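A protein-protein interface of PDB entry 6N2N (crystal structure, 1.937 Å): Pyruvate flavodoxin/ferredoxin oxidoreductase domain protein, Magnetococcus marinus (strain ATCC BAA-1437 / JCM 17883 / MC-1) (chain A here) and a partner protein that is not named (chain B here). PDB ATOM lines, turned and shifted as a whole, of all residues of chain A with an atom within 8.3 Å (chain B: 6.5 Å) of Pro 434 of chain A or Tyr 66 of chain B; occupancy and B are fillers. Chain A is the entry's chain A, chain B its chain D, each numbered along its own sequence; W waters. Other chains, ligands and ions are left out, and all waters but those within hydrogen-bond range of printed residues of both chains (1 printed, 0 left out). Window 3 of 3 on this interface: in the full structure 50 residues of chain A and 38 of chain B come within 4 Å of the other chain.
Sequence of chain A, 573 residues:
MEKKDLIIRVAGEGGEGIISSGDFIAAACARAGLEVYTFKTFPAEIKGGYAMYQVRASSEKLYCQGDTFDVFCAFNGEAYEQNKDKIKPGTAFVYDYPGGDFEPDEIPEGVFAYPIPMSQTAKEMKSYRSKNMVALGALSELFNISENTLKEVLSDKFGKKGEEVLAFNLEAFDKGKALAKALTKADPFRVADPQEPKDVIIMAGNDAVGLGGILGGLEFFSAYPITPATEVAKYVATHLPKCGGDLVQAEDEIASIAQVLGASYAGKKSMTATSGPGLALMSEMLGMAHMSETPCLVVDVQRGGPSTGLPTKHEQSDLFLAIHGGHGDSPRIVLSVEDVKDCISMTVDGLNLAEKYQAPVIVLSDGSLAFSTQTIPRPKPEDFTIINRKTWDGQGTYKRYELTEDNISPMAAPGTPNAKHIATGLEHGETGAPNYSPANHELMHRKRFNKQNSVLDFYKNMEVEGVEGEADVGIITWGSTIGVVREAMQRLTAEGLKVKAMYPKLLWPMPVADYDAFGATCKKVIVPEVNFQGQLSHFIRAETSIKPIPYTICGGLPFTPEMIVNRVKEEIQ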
ATOM      1  N   ILE A 422       4.981 -27.948   9.058  1.00  0.00           N
ATOM      2  CA  ILE A 422       4.976 -26.495   8.986  1.00  0.00           C
ATOM      3  C   ILE A 422       3.540 -26.009   9.129  1.00  0.00           C
ATOM      4  O   ILE A 422       2.610 -26.606   8.577  1.00  0.00           O
ATOM      5  CB  ILE A 422       5.616 -25.967   7.680  1.00  0.00           C
ATOM      6  CG1 ILE A 422       5.778 -24.446   7.750  1.00  0.00           C
ATOM      7  CG2 ILE A 422       4.771 -26.328   6.466  1.00  0.00           C
ATOM      8  CD1 ILE A 422       6.721 -23.889   6.703  1.00  0.00           C
ATOM      9  N   ALA A 423       3.355 -24.962   9.923  1.00  0.00           N
ATOM     10  CA  ALA A 423       2.143 -24.166   9.870  1.00  0.00           C
ATOM     11  C   ALA A 423       2.424 -22.958   8.989  1.00  0.00           C
ATOM     12  O   ALA A 423       3.488 -22.341   9.095  1.00  0.00           O
ATOM     13  CB  ALA A 423       1.703 -23.720  11.268  1.00  0.00           C
ATOM     14  N   THR A 424       1.485 -22.632   8.104  1.00  0.00           N
ATOM     15  CA  THR A 424       1.782 -21.641   7.080  1.00  0.00           C
ATOM     16  C   THR A 424       0.551 -20.801   6.759  1.00  0.00           C
ATOM     17  O   THR A 424      -0.586 -21.278   6.822  1.00  0.00           O
ATOM     18  CB  THR A 424       2.300 -22.299   5.795  1.00  0.00           C
ATOM     19  OG1 THR A 424       2.598 -21.280   4.832  1.00  0.00           O
ATOM     20  CG2 THR A 424       1.265 -23.253   5.219  1.00  0.00           C
ATOM     21  N   GLY A 425       0.808 -19.545   6.379  1.00  0.00           N
ATOM     22  CA  GLY A 425      -0.195 -18.623   5.879  1.00  0.00           C
ATOM     23  C   GLY A 425      -0.398 -18.654   4.377  1.00  0.00           C
ATOM     24  O   GLY A 425      -1.361 -18.070   3.876  1.00  0.00           O
ATOM     25  N   LEU A 426       0.485 -19.317   3.631  1.00  0.00           N
ATOM     26  CA  LEU A 426       0.205 -19.570   2.224  1.00  0.00           C
ATOM     27  C   LEU A 426      -0.880 -20.627   2.097  1.00  0.00           C
ATOM     28  O   LEU A 426      -0.979 -21.541   2.921  1.00  0.00           O
ATOM     29  CB  LEU A 426       1.465 -20.042   1.493  1.00  0.00           C
ATOM     30  CG  LEU A 426       2.480 -18.962   1.109  1.00  0.00           C
ATOM     31  CD1 LEU A 426       3.808 -19.599   0.719  1.00  0.00           C
ATOM     32  CD2 LEU A 426       1.940 -18.131  -0.047  1.00  0.00           C
ATOM     33  N   GLU A 427      -1.695 -20.510   1.050  1.00  0.00           N
ATOM     34  CA  GLU A 427      -2.590 -21.612   0.729  1.00  0.00           C
ATOM     35  C   GLU A 427      -1.754 -22.850   0.447  1.00  0.00           C
ATOM     36  O   GLU A 427      -0.650 -22.762  -0.093  1.00  0.00           O
ATOM     37  CB  GLU A 427      -3.484 -21.283  -0.464  1.00  0.00           C
ATOM     38  CG  GLU A 427      -4.517 -22.380  -0.776  1.00  0.00           C
ATOM     39  CD  GLU A 427      -5.502 -22.623   0.365  1.00  0.00           C
ATOM     40  OE1 GLU A 427      -6.650 -22.139   0.275  1.00  0.00           O
ATOM     41  OE2 GLU A 427      -5.132 -23.298   1.353  1.00  0.00           O
ATOM     42  N   HIS A 428      -2.270 -24.007   0.849  1.00  0.00           N
ATOM     43  CA  HIS A 428      -1.423 -25.173   1.030  1.00  0.00           C
ATOM     44  C   HIS A 428      -2.260 -26.430   0.882  1.00  0.00           C
ATOM     45  O   HIS A 428      -3.486 -26.399   1.008  1.00  0.00           O
ATOM     46  CB  HIS A 428      -0.766 -25.149   2.410  1.00  0.00           C
ATOM     47  CG  HIS A 428      -1.744 -24.918   3.516  1.00  0.00           C
ATOM     48  ND1 HIS A 428      -2.063 -23.658   3.973  1.00  0.00           N
ATOM     49  CD2 HIS A 428      -2.523 -25.781   4.213  1.00  0.00           C
ATOM     50  CE1 HIS A 428      -2.975 -23.756   4.927  1.00  0.00           C
ATOM     51  NE2 HIS A 428      -3.270 -25.034   5.091  1.00  0.00           N
ATOM     52  N   GLY A 429      -1.569 -27.545   0.644  1.00  0.00           N
ATOM     53  CA  GLY A 429      -2.189 -28.851   0.644  1.00  0.00           C
ATOM     54  C   GLY A 429      -2.118 -29.507   2.012  1.00  0.00           C
ATOM     55  O   GLY A 429      -1.788 -28.884   3.024  1.00  0.00           O
ATOM     56  N   GLU A 430      -2.407 -30.813   2.023  1.00  0.00           N
ATOM     57  CA  GLU A 430      -2.551 -31.552   3.278  1.00  0.00           C
ATOM     58  C   GLU A 430      -1.283 -31.545   4.122  1.00  0.00           C
ATOM     59  O   GLU A 430      -1.361 -31.619   5.355  1.00  0.00           O
ATOM     60  CB  GLU A 430      -2.948 -32.994   2.984  1.00  0.00           C
ATOM     61  CG  GLU A 430      -4.415 -33.218   2.797  1.00  0.00           C
ATOM     62  CD  GLU A 430      -4.743 -34.691   2.742  1.00  0.00           C
ATOM     63  OE1 GLU A 430      -4.304 -35.363   1.785  1.00  0.00           O
ATOM     64  OE2 GLU A 430      -5.389 -35.184   3.687  1.00  0.00           O
ATOM     65  N   THR A 431      -0.114 -31.479   3.496  1.00  0.00           N
ATOM     66  CA  THR A 431       1.133 -31.501   4.243  1.00  0.00           C
ATOM     67  C   THR A 431       1.632 -30.112   4.603  1.00  0.00           C
ATOM     68  O   THR A 431       2.682 -29.995   5.244  1.00  0.00           O
ATOM     69  CB  THR A 431       2.225 -32.215   3.439  1.00  0.00           C
ATOM     70  OG1 THR A 431       2.544 -31.430   2.283  1.00  0.00           O
ATOM     71  CG2 THR A 431       1.754 -33.598   3.005  1.00  0.00           C
ATOM     72  N   GLY A 432       0.898 -29.065   4.235  1.00  0.00           N
ATOM     73  CA  GLY A 432       1.345 -27.714   4.471  1.00  0.00           C
ATOM     74  C   GLY A 432       2.260 -27.154   3.408  1.00  0.00           C
ATOM     75  O   GLY A 432       2.757 -26.033   3.574  1.00  0.00           O
ATOM     76  N   ALA A 433       2.528 -27.902   2.338  1.00  0.00           N
ATOM     77  CA  ALA A 433       3.316 -27.350   1.251  1.00  0.00           C
ATOM     78  C   ALA A 433       2.470 -26.351   0.466  1.00  0.00           C
ATOM     79  O   ALA A 433       1.283 -26.597   0.234  1.00  0.00           O
ATOM     80  CB  ALA A 433       3.815 -28.460   0.324  1.00  0.00           C
ATOM     81  N   PRO A 434       3.052 -25.233   0.030  1.00  0.00           N
ATOM     82  CA  PRO A 434       2.275 -24.244  -0.724  1.00  0.00           C
ATOM     83  C   PRO A 434       1.635 -24.877  -1.949  1.00  0.00           C
ATOM     84  O   PRO A 434       2.236 -25.716  -2.628  1.00  0.00           O
ATOM     85  CB  PRO A 434       3.315 -23.185  -1.106  1.00  0.00           C
ATOM     86  CG  PRO A 434       4.441 -23.379  -0.136  1.00  0.00           C
ATOM     87  CD  PRO A 434       4.469 -24.851   0.147  1.00  0.00           C
ATOM     88  N   ASN A 435       0.388 -24.490  -2.207  1.00  0.00           N
ATOM     89  CA  ASN A 435      -0.410 -25.104  -3.263  1.00  0.00           C
ATOM     90  C   ASN A 435      -1.351 -24.045  -3.809  1.00  0.00           C
ATOM     91  O   ASN A 435      -2.224 -23.567  -3.080  1.00  0.00           O
ATOM     92  CB  ASN A 435      -1.191 -26.313  -2.718  1.00  0.00           C
ATOM     93  CG  ASN A 435      -1.932 -27.093  -3.802  1.00  0.00           C
ATOM     94  OD1 ASN A 435      -2.460 -26.517  -4.754  1.00  0.00           O
ATOM     95  ND2 ASN A 435      -1.999 -28.410  -3.638  1.00  0.00           N
ATOM     96  N   TYR A 436      -1.177 -23.677  -5.080  1.00  0.00           N
ATOM     97  CA  TYR A 436      -1.977 -22.622  -5.693  1.00  0.00           C
ATOM     98  C   TYR A 436      -2.987 -23.143  -6.705  1.00  0.00           C
ATOM     99  O   TYR A 436      -3.561 -22.343  -7.452  1.00  0.00           O
ATOM    100  CB  TYR A 436      -1.064 -21.588  -6.352  1.00  0.00           C
ATOM    101  CG  TYR A 436       0.052 -21.155  -5.437  1.00  0.00           C
ATOM    102  CD1 TYR A 436      -0.228 -20.559  -4.216  1.00  0.00           C
ATOM    103  CD2 TYR A 436       1.382 -21.361  -5.781  1.00  0.00           C
ATOM    104  CE1 TYR A 436       0.785 -20.169  -3.360  1.00  0.00           C
ATOM    105  CE2 TYR A 436       2.407 -20.968  -4.930  1.00  0.00           C
ATOM    106  CZ  TYR A 436       2.099 -20.374  -3.722  1.00  0.00           C
ATOM    107  OH  TYR A 436       3.106 -19.987  -2.872  1.00  0.00           O
ATOM    108  N   SER A 437      -3.241 -24.452  -6.733  1.00  0.00           N
ATOM    109  CA  SER A 437      -4.147 -24.997  -7.730  1.00  0.00           C
ATOM    110  C   SER A 437      -5.600 -24.657  -7.390  1.00  0.00           C
ATOM    111  O   SER A 437      -5.967 -24.537  -6.213  1.00  0.00           O
ATOM    112  CB  SER A 437      -3.972 -26.509  -7.855  1.00  0.00           C
ATOM    113  OG  SER A 437      -4.426 -27.185  -6.702  1.00  0.00           O
ATOM    114  N   ASN A 440      -7.518 -27.238  -5.086  1.00  0.00           N
ATOM    115  CA  ASN A 440      -7.080 -27.258  -3.695  1.00  0.00           C
ATOM    116  C   ASN A 440      -7.609 -26.051  -2.928  1.00  0.00           C
ATOM    117  O   ASN A 440      -8.042 -26.186  -1.781  1.00  0.00           O
ATOM    118  CB  ASN A 440      -5.557 -27.298  -3.616  1.00  0.00           C
ATOM    119  CG  ASN A 440      -5.050 -27.230  -2.187  1.00  0.00           C
ATOM    120  OD1 ASN A 440      -5.037 -28.231  -1.469  1.00  0.00           O
ATOM    121  ND2 ASN A 440      -4.640 -26.041  -1.763  1.00  0.00           N
ATOM    122  N   SER B  19      14.755 -31.196   3.882  1.00  0.00           N
ATOM    123  CA  SER B  19      13.425 -31.682   3.550  1.00  0.00           C
ATOM    124  C   SER B  19      13.410 -32.152   2.095  1.00  0.00           C
ATOM    125  O   SER B  19      14.412 -32.073   1.381  1.00  0.00           O
ATOM    126  CB  SER B  19      12.381 -30.595   3.785  1.00  0.00           C
ATOM    127  OG  SER B  19      12.410 -29.657   2.728  1.00  0.00           O
ATOM    128  N   GLU B  20      12.257 -32.647   1.644  1.00  0.00           N
ATOM    129  CA  GLU B  20      12.119 -33.079   0.256  1.00  0.00           C
ATOM    130  C   GLU B  20      11.834 -31.927  -0.700  1.00  0.00           C
ATOM    131  O   GLU B  20      11.848 -32.138  -1.918  1.00  0.00           O
ATOM    132  CB  GLU B  20      10.998 -34.115   0.120  1.00  0.00           C
ATOM    133  CG  GLU B  20       9.597 -33.528   0.212  1.00  0.00           C
ATOM    134  CD  GLU B  20       9.195 -33.123   1.621  1.00  0.00           C
ATOM    135  OE1 GLU B  20       8.037 -32.705   1.799  1.00  0.00           O
ATOM    136  OE2 GLU B  20      10.028 -33.219   2.545  1.00  0.00           O
ATOM    137  N   VAL B  21      11.582 -30.727  -0.187  1.00  0.00           N
ATOM    138  CA  VAL B  21      11.198 -29.590  -1.021  1.00  0.00           C
ATOM    139  C   VAL B  21      12.422 -29.157  -1.818  1.00  0.00           C
ATOM    140  O   VAL B  21      13.467 -28.852  -1.228  1.00  0.00           O
ATOM    141  CB  VAL B  21      10.649 -28.433  -0.166  1.00  0.00           C
ATOM    142  CG1 VAL B  21      10.221 -27.257  -1.046  1.00  0.00           C
ATOM    143  CG2 VAL B  21       9.497 -28.899   0.708  1.00  0.00           C
ATOM    144  N   SER B  56      10.048 -18.118  10.029  1.00  0.00           N
ATOM    145  CA  SER B  56      10.404 -17.081   9.071  1.00  0.00           C
ATOM    146  C   SER B  56       9.185 -16.233   8.734  1.00  0.00           C
ATOM    147  O   SER B  56       8.041 -16.591   9.040  1.00  0.00           O
ATOM    148  CB  SER B  56      10.979 -17.678   7.784  1.00  0.00           C
ATOM    149  OG  SER B  56       9.991 -18.443   7.130  1.00  0.00           O
ATOM    150  N   SER B  62      13.187 -15.968   3.481  1.00  0.00           N
ATOM    151  CA  SER B  62      12.197 -16.559   4.376  1.00  0.00           C
ATOM    152  C   SER B  62      11.681 -17.907   3.899  1.00  0.00           C
ATOM    153  O   SER B  62      10.972 -18.576   4.657  1.00  0.00           O
ATOM    154  CB  SER B  62      11.015 -15.603   4.554  1.00  0.00           C
ATOM    155  OG  SER B  62      11.440 -14.361   5.077  1.00  0.00           O
ATOM    156  N   ARG B  63      11.997 -18.320   2.671  1.00  0.00           N
ATOM    157  CA  ARG B  63      11.619 -19.658   2.238  1.00  0.00           C
ATOM    158  C   ARG B  63      12.438 -20.743   2.923  1.00  0.00           C
ATOM    159  O   ARG B  63      12.057 -21.917   2.849  1.00  0.00           O
ATOM    160  CB  ARG B  63      11.756 -19.773   0.717  1.00  0.00           C
ATOM    161  CG  ARG B  63      11.004 -18.688  -0.064  1.00  0.00           C
ATOM    162  CD  ARG B  63      11.304 -18.792  -1.551  1.00  0.00           C
ATOM    163  NE  ARG B  63      10.979 -20.126  -2.045  1.00  0.00           N
ATOM    164  CZ  ARG B  63      11.395 -20.634  -3.200  1.00  0.00           C
ATOM    165  NH1 ARG B  63      12.171 -19.928  -4.017  1.00  0.00           N
ATOM    166  NH2 ARG B  63      11.038 -21.868  -3.536  1.00  0.00           N
ATOM    167  N   MET B  64      13.520 -20.379   3.615  1.00  0.00           N
ATOM    168  CA  MET B  64      14.430 -21.378   4.173  1.00  0.00           C
ATOM    169  C   MET B  64      13.762 -22.457   5.024  1.00  0.00           C
ATOM    170  O   MET B  64      14.121 -23.634   4.857  1.00  0.00           O
ATOM    171  CB  MET B  64      15.515 -20.710   5.034  1.00  0.00           C
ATOM    172  CG  MET B  64      16.655 -21.684   5.385  1.00  0.00           C
ATOM    173  SD  MET B  64      17.793 -21.139   6.668  1.00  0.00           S
ATOM    174  CE  MET B  64      16.779 -21.446   8.118  1.00  0.00           C
ATOM    175  N   PRO B  65      12.822 -22.159   5.930  1.00  0.00           N
ATOM    176  CA  PRO B  65      12.258 -23.243   6.755  1.00  0.00           C
ATOM    177  C   PRO B  65      11.605 -24.361   5.962  1.00  0.00           C
ATOM    178  O   PRO B  65      11.614 -25.505   6.432  1.00  0.00           O
ATOM    179  CB  PRO B  65      11.237 -22.514   7.635  1.00  0.00           C
ATOM    180  CG  PRO B  65      11.769 -21.141   7.738  1.00  0.00           C
ATOM    181  CD  PRO B  65      12.350 -20.839   6.395  1.00  0.00           C
ATOM    182  N   TYR B  66      11.053 -24.074   4.776  1.00  0.00           N
ATOM    183  CA  TYR B  66      10.497 -25.144   3.949  1.00  0.00           C
ATOM    184  C   TYR B  66      11.544 -26.201   3.628  1.00  0.00           C
ATOM    185  O   TYR B  66      11.210 -27.382   3.485  1.00  0.00           O
ATOM    186  CB  TYR B  66       9.921 -24.587   2.646  1.00  0.00           C
ATOM    187  CG  TYR B  66       8.626 -23.834   2.820  1.00  0.00           C
ATOM    188  CD1 TYR B  66       7.418 -24.511   2.953  1.00  0.00           C
ATOM    189  CD2 TYR B  66       8.609 -22.448   2.829  1.00  0.00           C
ATOM    190  CE1 TYR B  66       6.222 -23.823   3.117  1.00  0.00           C
ATOM    191  CE2 TYR B  66       7.422 -21.748   2.988  1.00  0.00           C
ATOM    192  CZ  TYR B  66       6.233 -22.442   3.132  1.00  0.00           C
ATOM    193  OH  TYR B  66       5.061 -21.747   3.287  1.00  0.00           O
ATOM    194  N   PHE B  67      12.809 -25.801   3.526  1.00  0.00           N
ATOM    195  CA  PHE B  67      13.891 -26.692   3.130  1.00  0.00           C
ATOM    196  C   PHE B  67      14.526 -27.428   4.305  1.00  0.00           C
ATOM    197  O   PHE B  67      15.500 -28.157   4.106  1.00  0.00           O
ATOM    198  CB  PHE B  67      14.980 -25.903   2.393  1.00  0.00           C
ATOM    199  CG  PHE B  67      14.461 -24.980   1.317  1.00  0.00           C
ATOM    200  CD1 PHE B  67      13.465 -25.391   0.443  1.00  0.00           C
ATOM    201  CD2 PHE B  67      14.998 -23.711   1.161  1.00  0.00           C
ATOM    202  CE1 PHE B  67      13.002 -24.553  -0.553  1.00  0.00           C
ATOM    203  CE2 PHE B  67      14.540 -22.861   0.166  1.00  0.00           C
ATOM    204  CZ  PHE B  67      13.541 -23.284  -0.696  1.00  0.00           C
ATOM    205  N   VAL B  68      14.011 -27.258   5.518  1.00  0.00           N
ATOM    206  CA  VAL B  68      14.607 -27.837   6.715  1.00  0.00           C
ATOM    207  C   VAL B  68      13.651 -28.873   7.279  1.00  0.00           C
ATOM    208  O   VAL B  68      12.454 -28.600   7.443  1.00  0.00           O
ATOM    209  CB  VAL B  68      14.918 -26.752   7.765  1.00  0.00           C
ATOM    210  CG1 VAL B  68      15.540 -27.371   9.008  1.00  0.00           C
ATOM    211  CG2 VAL B  68      15.828 -25.689   7.180  1.00  0.00           C
ATOM    212  N   ASP B  69      14.174 -30.056   7.585  1.00  0.00           N
ATOM    213  CA  ASP B  69      13.367 -31.109   8.197  1.00  0.00           C
ATOM    214  C   ASP B  69      13.366 -30.883   9.703  1.00  0.00           C
ATOM    215  O   ASP B  69      14.290 -31.297  10.408  1.00  0.00           O
ATOM    216  CB  ASP B  69      13.901 -32.489   7.836  1.00  0.00           C
ATOM    217  CG  ASP B  69      13.192 -33.587   8.596  1.00  0.00           C
ATOM    218  OD1 ASP B  69      11.995 -33.808   8.326  1.00  0.00           O
ATOM    219  OD2 ASP B  69      13.829 -34.226   9.465  1.00  0.00           O
ATOM    220  N   LYS B  72       8.453 -26.085  12.112  1.00  0.00           N
ATOM    221  CA  LYS B  72       8.637 -24.828  11.400  1.00  0.00           C
ATOM    222  C   LYS B  72       7.320 -24.069  11.268  1.00  0.00           C
ATOM    223  O   LYS B  72       6.232 -24.647  11.345  1.00  0.00           O
ATOM    224  CB  LYS B  72       9.286 -25.111  10.041  1.00  0.00           C
ATOM    225  CG  LYS B  72       8.610 -26.260   9.328  1.00  0.00           C
ATOM    226  CD  LYS B  72       9.518 -26.933   8.311  1.00  0.00           C
ATOM    227  CE  LYS B  72       8.945 -28.279   7.873  1.00  0.00           C
ATOM    228  NZ  LYS B  72       9.745 -28.851   6.751  1.00  0.00           N
ATOM    229  N   HIS B  74       5.881 -20.760   8.664  1.00  0.00           N
ATOM    230  CA  HIS B  74       5.989 -19.685   7.684  1.00  0.00           C
ATOM    231  C   HIS B  74       4.903 -18.680   8.041  1.00  0.00           C
ATOM    232  O   HIS B  74       3.719 -18.938   7.801  1.00  0.00           O
ATOM    233  CB  HIS B  74       5.787 -20.186   6.257  1.00  0.00           C
ATOM    234  CG  HIS B  74       6.204 -19.199   5.210  1.00  0.00           C
ATOM    235  ND1 HIS B  74       5.674 -19.191   3.938  1.00  0.00           N
ATOM    236  CD2 HIS B  74       7.133 -18.215   5.234  1.00  0.00           C
ATOM    237  CE1 HIS B  74       6.237 -18.226   3.233  1.00  0.00           C
ATOM    238  NE2 HIS B  74       7.130 -17.622   3.995  1.00  0.00           N
HETATM  239  O   HOH W   1       2.994 -17.250   5.296  1.00  0.00           O
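Among the printed residues, merely in contact across the chains: Ile 422 of chain A with Lys 72 of chain B (3.2 Å), Thr 424 of chain A with His 74 of chain B (3.4 Å), Leu 426 of chain A with Tyr 66 of chain B (3.6 Å), Pro 434 of chain A with Tyr 66 of chain B (3.6 Å), Ile 422 of chain A with Tyr 66 of chain B (3.6 Å), Leu 426 of chain A with His 74 of chain B (3.7 Å) and Ile 422 of chain A with His 74 of chain B (3.8 Å).
Pro 434 of chain A touches just one residue of chain B: Tyr 66 (3.6 Å). Tyr 66 of chain B touches just these residues of chain A: Ile 422 (3.6 Å), Thr 424 (2.9 Å), Leu 426 (3.6 Å) and Pro 434 (3.6 Å). No residue of chain A comes within 4 Å of Pro 65 of chain B. Printed residues of chain A within 4 Å of Lys 72 of chain B: Ile 422 and Ala 423. Printed residues of chain A within 4 Å of His 74 of chain B: Ile 422, Ala 423, Thr 424, Gly 425 and Leu 426. Thr 431 of chain A touches none of the printed residues of chain B. Ser 56 of chain B touches none of the printed residues of chain A. The nearest printed residue of chain A that does not touch Lys 72 of chain B is Thr 424 of chain A (6.1 Å).
Water W1 lies within hydrogen-bond range of the backbone carbonyl oxygen (O) of His 74 of chain B (3.1 Å) and the backbone NH (N) of Gly 425 of chain A (3.3 Å).
The backbone carbonyl oxygen (O) of Lys 72 of chain B lies within hydrogen-bond range of the backbone NH (N) of Ala 423 of chain A (3.2 Å). O of Ala 423 of chain A sits at hydrogen-bond distance from N of His 74 of chain B. OG1 of Thr 424 of chain A sits at hydrogen-bond distance from OH of Tyr 66 of chain B. O of His 74 of chain B is in hydrogen-bond range of N of Gly 425 of chain A.
Of the 17 printed residues of chain A, 6 touch a printed residue of chain B. Printed residues of chain A that touch a printed residue of chain B: Ile 422, Ala 423, Thr 424, Gly 425, Leu 426 and Pro 434. Among the printed residues, no Asp or Glu carboxylate lies within 4 Å of a Lys or Arg side-chain nitrogen of the other chain.
The backbone NH of Leu 426 of chain A sits at hydrogen-bond distance from the side-chain hydroxyl of Thr 424 of chain A (3.1 Å). ND1 of His 428 of chain A sits at hydrogen-bond distance from O of Leu 426 of chain A. OG of Ser 19 of chain B is in hydrogen-bond range of O of Tyr 66 of chain B. The side-chain hydroxyl of Tyr 66 of chain B is in hydrogen-bond range of a ring nitrogen (ND1) of His 74 of chain B (2.7 Å). The backbone carbonyl oxygen (O) of Val 68 of chain B lies within hydrogen-bond range of the side-chain amino group (NZ) of Lys 72 of chain B (2.8 Å).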
